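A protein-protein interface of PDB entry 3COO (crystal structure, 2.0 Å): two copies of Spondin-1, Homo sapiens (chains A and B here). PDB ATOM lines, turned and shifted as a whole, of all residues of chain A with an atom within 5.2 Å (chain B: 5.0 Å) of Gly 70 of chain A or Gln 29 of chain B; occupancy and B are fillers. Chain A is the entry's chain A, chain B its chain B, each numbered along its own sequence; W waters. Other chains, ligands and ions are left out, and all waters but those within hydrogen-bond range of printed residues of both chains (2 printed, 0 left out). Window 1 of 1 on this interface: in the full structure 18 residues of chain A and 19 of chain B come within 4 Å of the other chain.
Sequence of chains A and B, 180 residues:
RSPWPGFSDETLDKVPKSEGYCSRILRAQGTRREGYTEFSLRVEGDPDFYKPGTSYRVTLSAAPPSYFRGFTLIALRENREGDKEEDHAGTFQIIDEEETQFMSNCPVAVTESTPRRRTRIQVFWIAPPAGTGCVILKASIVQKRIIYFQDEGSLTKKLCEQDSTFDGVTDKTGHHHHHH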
ATOM      1  N   TYR A  67      21.559 -23.925   4.267  1.00  0.00           N
ATOM      2  CA  TYR A  67      22.420 -22.752   4.066  1.00  0.00           C
ATOM      3  C   TYR A  67      23.123 -22.504   5.382  1.00  0.00           C
ATOM      4  O   TYR A  67      22.687 -22.986   6.438  1.00  0.00           O
ATOM      5  CB  TYR A  67      21.593 -21.487   3.604  1.00  0.00           C
ATOM      6  CG  TYR A  67      20.719 -20.865   4.700  1.00  0.00           C
ATOM      7  CD1 TYR A  67      21.226 -19.900   5.571  1.00  0.00           C
ATOM      8  CD2 TYR A  67      19.400 -21.270   4.876  1.00  0.00           C
ATOM      9  CE1 TYR A  67      20.434 -19.347   6.617  1.00  0.00           C
ATOM     10  CE2 TYR A  67      18.577 -20.716   5.897  1.00  0.00           C
ATOM     11  CZ  TYR A  67      19.101 -19.772   6.771  1.00  0.00           C
ATOM     12  OH  TYR A  67      18.293 -19.264   7.777  1.00  0.00           O
ATOM     13  N   PHE A  68      24.215 -21.754   5.324  1.00  0.00           N
ATOM     14  CA  PHE A  68      24.851 -21.249   6.548  1.00  0.00           C
ATOM     15  C   PHE A  68      25.086 -19.755   6.362  1.00  0.00           C
ATOM     16  O   PHE A  68      25.068 -19.256   5.241  1.00  0.00           O
ATOM     17  CB  PHE A  68      26.176 -21.977   6.863  1.00  0.00           C
ATOM     18  CG  PHE A  68      27.186 -21.976   5.734  1.00  0.00           C
ATOM     19  CD1 PHE A  68      27.097 -22.904   4.710  1.00  0.00           C
ATOM     20  CD2 PHE A  68      28.245 -21.064   5.714  1.00  0.00           C
ATOM     21  CE1 PHE A  68      28.031 -22.935   3.662  1.00  0.00           C
ATOM     22  CE2 PHE A  68      29.186 -21.081   4.684  1.00  0.00           C
ATOM     23  CZ  PHE A  68      29.092 -22.029   3.655  1.00  0.00           C
ATOM     24  N   ARG A  69      25.255 -19.035   7.456  1.00  0.00           N
ATOM     25  CA  ARG A  69      25.688 -17.643   7.354  1.00  0.00           C
ATOM     26  C   ARG A  69      27.184 -17.574   7.691  1.00  0.00           C
ATOM     27  O   ARG A  69      28.021 -17.683   6.802  1.00  0.00           O
ATOM     28  CB  ARG A  69      24.797 -16.756   8.254  1.00  0.00           C
ATOM     29  CG  ARG A  69      23.317 -16.788   7.869  1.00  0.00           C
ATOM     30  CD  ARG A  69      22.555 -15.878   8.806  1.00  0.00           C
ATOM     31  NE  ARG A  69      21.131 -15.795   8.529  1.00  0.00           N
ATOM     32  CZ  ARG A  69      20.570 -14.845   7.782  1.00  0.00           C
ATOM     33  NH1 ARG A  69      21.356 -13.952   7.214  1.00  0.00           N
ATOM     34  NH2 ARG A  69      19.234 -14.792   7.600  1.00  0.00           N
ATOM     35  N   GLY A  70      27.562 -17.531   8.958  1.00  0.00           N
ATOM     36  CA  GLY A  70      28.989 -17.446   9.268  1.00  0.00           C
ATOM     37  C   GLY A  70      29.629 -18.848   9.317  1.00  0.00           C
ATOM     38  O   GLY A  70      28.944 -19.890   9.346  1.00  0.00           O
ATOM     39  N   PHE A  71      30.944 -18.880   9.337  1.00  0.00           N
ATOM     40  CA  PHE A  71      31.634 -20.149   9.494  1.00  0.00           C
ATOM     41  C   PHE A  71      33.037 -19.781   9.963  1.00  0.00           C
ATOM     42  O   PHE A  71      33.469 -18.636   9.770  1.00  0.00           O
ATOM     43  CB  PHE A  71      31.769 -20.864   8.119  1.00  0.00           C
ATOM     44  CG  PHE A  71      32.591 -20.093   7.136  1.00  0.00           C
ATOM     45  CD1 PHE A  71      32.005 -19.078   6.373  1.00  0.00           C
ATOM     46  CD2 PHE A  71      33.976 -20.348   7.019  1.00  0.00           C
ATOM     47  CE1 PHE A  71      32.779 -18.334   5.477  1.00  0.00           C
ATOM     48  CE2 PHE A  71      34.750 -19.611   6.153  1.00  0.00           C
ATOM     49  CZ  PHE A  71      34.169 -18.602   5.402  1.00  0.00           C
ATOM     50  N   THR A  72      33.748 -20.766  10.533  1.00  0.00           N
ATOM     51  CA  THR A  72      35.154 -20.593  10.826  1.00  0.00           C
ATOM     52  C   THR A  72      35.906 -21.818  10.323  1.00  0.00           C
ATOM     53  O   THR A  72      35.478 -22.933  10.609  1.00  0.00           O
ATOM     54  CB  THR A  72      35.415 -20.429  12.376  1.00  0.00           C
ATOM     55  OG1 THR A  72      34.571 -19.413  12.918  1.00  0.00           O
ATOM     56  CG2 THR A  72      36.879 -20.014  12.613  1.00  0.00           C
ATOM     57  N   GLU A 112      33.717 -15.717   7.627  1.00  0.00           N
ATOM     58  CA  GLU A 112      32.941 -14.846   6.741  1.00  0.00           C
ATOM     59  C   GLU A 112      33.273 -13.365   7.055  1.00  0.00           C
ATOM     60  O   GLU A 112      33.762 -13.066   8.130  1.00  0.00           O
ATOM     61  CB  GLU A 112      31.443 -15.122   6.950  1.00  0.00           C
ATOM     62  CG  GLU A 112      30.831 -14.382   8.202  1.00  0.00           C
ATOM     63  CD  GLU A 112      31.197 -14.979   9.551  1.00  0.00           C
ATOM     64  OE1 GLU A 112      30.832 -14.357  10.552  1.00  0.00           O
ATOM     65  OE2 GLU A 112      31.821 -16.053   9.658  1.00  0.00           O
ATOM     66  N   PRO A 115      27.131 -11.697   7.426  1.00  0.00           N
ATOM     67  CA  PRO A 115      26.314 -12.871   7.731  1.00  0.00           C
ATOM     68  C   PRO A 115      25.362 -13.201   6.561  1.00  0.00           C
ATOM     69  O   PRO A 115      24.303 -13.723   6.786  1.00  0.00           O
ATOM     70  CB  PRO A 115      25.513 -12.408   8.966  1.00  0.00           C
ATOM     71  CG  PRO A 115      25.323 -10.970   8.763  1.00  0.00           C
ATOM     72  CD  PRO A 115      26.470 -10.455   7.894  1.00  0.00           C
ATOM     73  N   ARG A 118      24.494 -18.369   2.582  1.00  0.00           N
ATOM     74  CA  ARG A 118      25.456 -18.957   1.641  1.00  0.00           C
ATOM     75  C   ARG A 118      25.184 -20.441   1.499  1.00  0.00           C
ATOM     76  O   ARG A 118      24.795 -21.105   2.476  1.00  0.00           O
ATOM     77  CB  ARG A 118      26.868 -18.894   2.256  1.00  0.00           C
ATOM     78  CG  ARG A 118      27.518 -17.556   2.162  1.00  0.00           C
ATOM     79  CD  ARG A 118      28.650 -17.455   3.166  1.00  0.00           C
ATOM     80  NE  ARG A 118      29.238 -16.129   3.041  1.00  0.00           N
ATOM     81  CZ  ARG A 118      29.040 -15.094   3.847  1.00  0.00           C
ATOM     82  NH1 ARG A 118      28.296 -15.189   4.954  1.00  0.00           N
ATOM     83  NH2 ARG A 118      29.640 -13.947   3.539  1.00  0.00           N
ATOM     84  N   SER A 140      33.750 -24.989  11.476  1.00  0.00           N
ATOM     85  CA  SER A 140      32.632 -24.951  12.411  1.00  0.00           C
ATOM     86  C   SER A 140      31.560 -23.998  11.881  1.00  0.00           C
ATOM     87  O   SER A 140      31.888 -22.958  11.303  1.00  0.00           O
ATOM     88  CB  SER A 140      33.101 -24.499  13.789  1.00  0.00           C
ATOM     89  OG  SER A 140      31.996 -24.147  14.575  1.00  0.00           O
ATOM     90  N   ILE A 141      30.302 -24.391  12.050  1.00  0.00           N
ATOM     91  CA  ILE A 141      29.132 -23.703  11.509  1.00  0.00           C
ATOM     92  C   ILE A 141      28.321 -23.121  12.712  1.00  0.00           C
ATOM     93  O   ILE A 141      27.329 -22.423  12.550  1.00  0.00           O
ATOM     94  CB  ILE A 141      28.339 -24.764  10.653  1.00  0.00           C
ATOM     95  CG1 ILE A 141      28.466 -24.497   9.161  1.00  0.00           C
ATOM     96  CG2 ILE A 141      26.982 -25.076  11.125  1.00  0.00           C
ATOM     97  CD1 ILE A 141      29.776 -24.100   8.793  1.00  0.00           C
ATOM     98  N   VAL A 142      28.802 -23.413  13.907  1.00  0.00           N
ATOM     99  CA  VAL A 142      28.199 -22.899  15.148  1.00  0.00           C
ATOM    100  C   VAL A 142      28.863 -21.572  15.552  1.00  0.00           C
ATOM    101  O   VAL A 142      30.067 -21.456  15.773  1.00  0.00           O
ATOM    102  CB  VAL A 142      28.224 -23.948  16.270  1.00  0.00           C
ATOM    103  CG1 VAL A 142      27.494 -25.222  15.825  1.00  0.00           C
ATOM    104  CG2 VAL A 142      29.642 -24.255  16.719  1.00  0.00           C
ATOM    105  N   GLN A 143      28.050 -20.556  15.583  1.00  0.00           N
ATOM    106  CA  GLN A 143      28.479 -19.196  15.678  1.00  0.00           C
ATOM    107  C   GLN A 143      28.289 -18.724  17.137  1.00  0.00           C
ATOM    108  O   GLN A 143      27.217 -18.264  17.452  1.00  0.00           O
ATOM    109  CB  GLN A 143      27.543 -18.437  14.741  1.00  0.00           C
ATOM    110  CG  GLN A 143      27.674 -18.919  13.271  1.00  0.00           C
ATOM    111  CD  GLN A 143      29.090 -18.725  12.820  1.00  0.00           C
ATOM    112  OE1 GLN A 143      29.550 -17.592  12.726  1.00  0.00           O
ATOM    113  NE2 GLN A 143      29.801 -19.806  12.577  1.00  0.00           N
ATOM    114  N   ARG B  27      17.652 -22.881  12.469  1.00  0.00           N
ATOM    115  CA  ARG B  27      18.253 -22.904  13.800  1.00  0.00           C
ATOM    116  C   ARG B  27      19.604 -23.543  13.818  1.00  0.00           C
ATOM    117  O   ARG B  27      20.161 -23.779  14.913  1.00  0.00           O
ATOM    118  CB  ARG B  27      17.320 -23.601  14.799  1.00  0.00           C
ATOM    119  CG  ARG B  27      16.111 -22.730  15.140  1.00  0.00           C
ATOM    120  CD  ARG B  27      14.800 -23.529  15.268  1.00  0.00           C
ATOM    121  NE  ARG B  27      14.784 -24.415  16.429  1.00  0.00           N
ATOM    122  CZ  ARG B  27      14.777 -25.749  16.384  1.00  0.00           C
ATOM    123  NH1 ARG B  27      14.767 -26.437  17.522  1.00  0.00           N
ATOM    124  NH2 ARG B  27      14.775 -26.405  15.222  1.00  0.00           N
ATOM    125  N   ALA B  28      20.131 -23.827  12.621  1.00  0.00           N
ATOM    126  CA  ALA B  28      21.318 -24.673  12.508  1.00  0.00           C
ATOM    127  C   ALA B  28      22.520 -24.059  13.232  1.00  0.00           C
ATOM    128  O   ALA B  28      23.281 -24.748  13.878  1.00  0.00           O
ATOM    129  CB  ALA B  28      21.660 -25.004  11.033  1.00  0.00           C
ATOM    130  N   GLN B  29      22.630 -22.736  13.148  1.00  0.00           N
ATOM    131  CA  GLN B  29      23.763 -22.020  13.721  1.00  0.00           C
ATOM    132  C   GLN B  29      23.316 -21.194  14.933  1.00  0.00           C
ATOM    133  O   GLN B  29      24.010 -20.253  15.322  1.00  0.00           O
ATOM    134  CB  GLN B  29      24.280 -21.056  12.648  1.00  0.00           C
ATOM    135  CG  GLN B  29      24.481 -21.699  11.304  1.00  0.00           C
ATOM    136  CD  GLN B  29      25.237 -20.793  10.390  1.00  0.00           C
ATOM    137  OE1 GLN B  29      24.638 -20.008   9.668  1.00  0.00           O
ATOM    138  NE2 GLN B  29      26.561 -20.843  10.461  1.00  0.00           N
ATOM    139  N   GLY B  30      22.145 -21.520  15.486  1.00  0.00           N
ATOM    140  CA  GLY B  30      21.450 -20.606  16.359  1.00  0.00           C
ATOM    141  C   GLY B  30      21.889 -20.676  17.817  1.00  0.00           C
ATOM    142  O   GLY B  30      22.355 -21.708  18.281  1.00  0.00           O
ATOM    143  N   THR B  31      21.775 -19.539  18.491  1.00  0.00           N
ATOM    144  CA  THR B  31      21.926 -19.445  19.938  1.00  0.00           C
ATOM    145  C   THR B  31      20.541 -19.194  20.534  1.00  0.00           C
ATOM    146  O   THR B  31      19.941 -18.158  20.282  1.00  0.00           O
ATOM    147  CB  THR B  31      22.847 -18.274  20.342  1.00  0.00           C
ATOM    148  OG1 THR B  31      24.185 -18.541  19.877  1.00  0.00           O
ATOM    149  CG2 THR B  31      22.843 -18.079  21.895  1.00  0.00           C
ATOM    150  N   ARG B 145      27.655 -12.104  14.086  1.00  0.00           N
ATOM    151  CA  ARG B 145      27.905 -13.540  13.809  1.00  0.00           C
ATOM    152  C   ARG B 145      26.799 -14.409  14.470  1.00  0.00           C
ATOM    153  O   ARG B 145      26.291 -15.350  13.890  1.00  0.00           O
ATOM    154  CB  ARG B 145      29.266 -13.995  14.353  1.00  0.00           C
ATOM    155  CG  ARG B 145      30.476 -13.303  13.744  1.00  0.00           C
ATOM    156  CD  ARG B 145      31.734 -14.093  14.010  1.00  0.00           C
ATOM    157  NE  ARG B 145      31.883 -15.160  13.023  1.00  0.00           N
ATOM    158  CZ  ARG B 145      32.658 -16.234  13.186  1.00  0.00           C
ATOM    159  NH1 ARG B 145      33.353 -16.421  14.311  1.00  0.00           N
ATOM    160  NH2 ARG B 145      32.710 -17.141  12.237  1.00  0.00           N
ATOM    161  N   ILE B 147      23.430 -15.920  15.708  1.00  0.00           N
ATOM    162  CA  ILE B 147      22.004 -15.961  15.271  1.00  0.00           C
ATOM    163  C   ILE B 147      21.157 -16.399  16.471  1.00  0.00           C
ATOM    164  O   ILE B 147      21.365 -17.510  17.010  1.00  0.00           O
ATOM    165  CB  ILE B 147      21.797 -16.990  14.121  1.00  0.00           C
ATOM    166  CG1 ILE B 147      22.636 -16.598  12.889  1.00  0.00           C
ATOM    167  CG2 ILE B 147      20.313 -17.179  13.800  1.00  0.00           C
ATOM    168  CD1 ILE B 147      23.268 -17.738  12.247  1.00  0.00           C
HETATM  169  O   HOH W   1      24.660 -18.380  17.136  1.00  0.00           O
HETATM  170  O   HOH W   2      26.675 -16.184  11.202  1.00  0.00           O
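The side-chain carboxylate (OE1) of Glu 112 of chain A is in salt-bridge range of the guanidinium group (NE) of Arg 145 of chain B (2.8 Å).
O of Phe 71 of chain A lies within hydrogen-bond range of NH2 of Arg 145 of chain B (3.0 Å).
The guanidinium group (NH2) of Arg 145 of chain B lies within hydrogen-bond range of the side-chain amide oxygen (OE1) of Gln 143 of chain A, at 3.2 Å.
OG1 of Thr 72 of chain A lies within hydrogen-bond range of NH2 of Arg 145 of chain B, 3.0 Å away.
The backbone carbonyl oxygen (O) of Gly 70 of chain A sits at hydrogen-bond distance from the side-chain amide nitrogen (NE2) of Gln 29 of chain B (2.8 Å).
O of Ile 141 of chain A sits at hydrogen-bond distance from NE2 of Gln 29 of chain B (2.7 Å).
The backbone NH (N) of Arg 69 of chain A lies within hydrogen-bond range of the side-chain amide oxygen (OE1) of Gln 29 of chain B (2.5 Å).
N of Ser 140 of chain A sits at hydrogen-bond distance from O of Thr 72 of chain A.
The backbone carbonyl oxygen (O) of Gly 70 of chain A is in hydrogen-bond range of the side-chain amide nitrogen (NE2) of Gln 143 of chain A (3.3 Å).
The backbone carbonyl oxygen (O) of Ile 147 of chain B sits at hydrogen-bond distance from the backbone NH (N) of Thr 31 of chain B (2.5 Å).
The guanidinium group of Arg 69 of chain A sits at hydrogen-bond distance from the backbone carbonyl oxygen of Pro 115 of chain A (3.0 Å).
OE2 of Glu 112 of chain A is in hydrogen-bond range of N of Phe 71 of chain A (3.0 Å).
The guanidinium group (NH1) of Arg 118 of chain A sits at hydrogen-bond distance from the backbone carbonyl oxygen (O) of Arg 69 of chain A, at 3.1 Å.
Among the printed residues, pairs that only touch across the chains: Phe 68 of chain A with Gln 29 of chain B (3.3 Å), Gln 143 of chain A with Gln 29 of chain B (3.6 Å), Gln 143 of chain A with Thr 31 of chain B (3.9 Å) and Arg 69 of chain A with Ile 147 of chain B (3.98 Å).
Of the printed residues of chain B, Arg 69 of chain A touches Gln 29 (2.5 Å) and Ile 147 (3.98 Å).
Gly 70 of chain A touches one residue of chain B.
Printed residues of chain B within 4 Å of Thr 72 of chain A: Arg 145.
Val 142 of chain A touches none of the printed residues of chain B.
Of the printed residues of chain B, Gln 143 of chain A touches Gln 29 (3.6 Å), Thr 31 (3.9 Å) and Arg 145 (3.2 Å).
Printed residues of chain A within 4 Å of Thr 31 of chain B: Gln 143 (3.9 Å).
The nearest residue of chain B that does not touch Gly 70 of chain A is Arg 145 of chain B (4.6 Å).
The nearest printed residue of chain A that does not touch Arg 145 of chain B is Gly 70 of chain A (4.6 Å).
Of the 13 printed residues of chain A, 8 touch a printed residue of chain B.
Printed residues of chain A that touch a printed residue of chain B: Phe 68, Arg 69, Gly 70, Phe 71, Thr 72, Glu 112, Ile 141 and Gln 143.
Of the 7 printed residues of chain B, 4 touch a printed residue of chain A.
Printed residues of chain B that touch a printed residue of chain A: Gln 29, Thr 31, Arg 145 and Ile 147.
Hydrophobic or aromatic side chains of chain B within 4 Å of the printed part of chain A: Ile 147.
Among the printed residues, 11 pairs touch across the chains.
No position is printed for both chains.
Of the 11 pairs that touch across the chains among the printed residues, none has its exchanged pair printed and touching as well.
Water W1 lies within hydrogen-bond range of the backbone carbonyl oxygen (O) of Gln 143 of chain A (2.6 Å), the backbone carbonyl oxygen (O) of Gln 29 of chain B (2.7 Å), the side-chain hydroxyl (OG1) of Thr 31 of chain B (2.8 Å) and the backbone NH (N) of Ile 147 of chain B (3.1 Å).
Water W2 lies within hydrogen-bond range of the backbone NH (N) of Gly 70 of chain A (2.8 Å) and the backbone carbonyl oxygen (O) of Arg 145 of chain B (2.8 Å).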
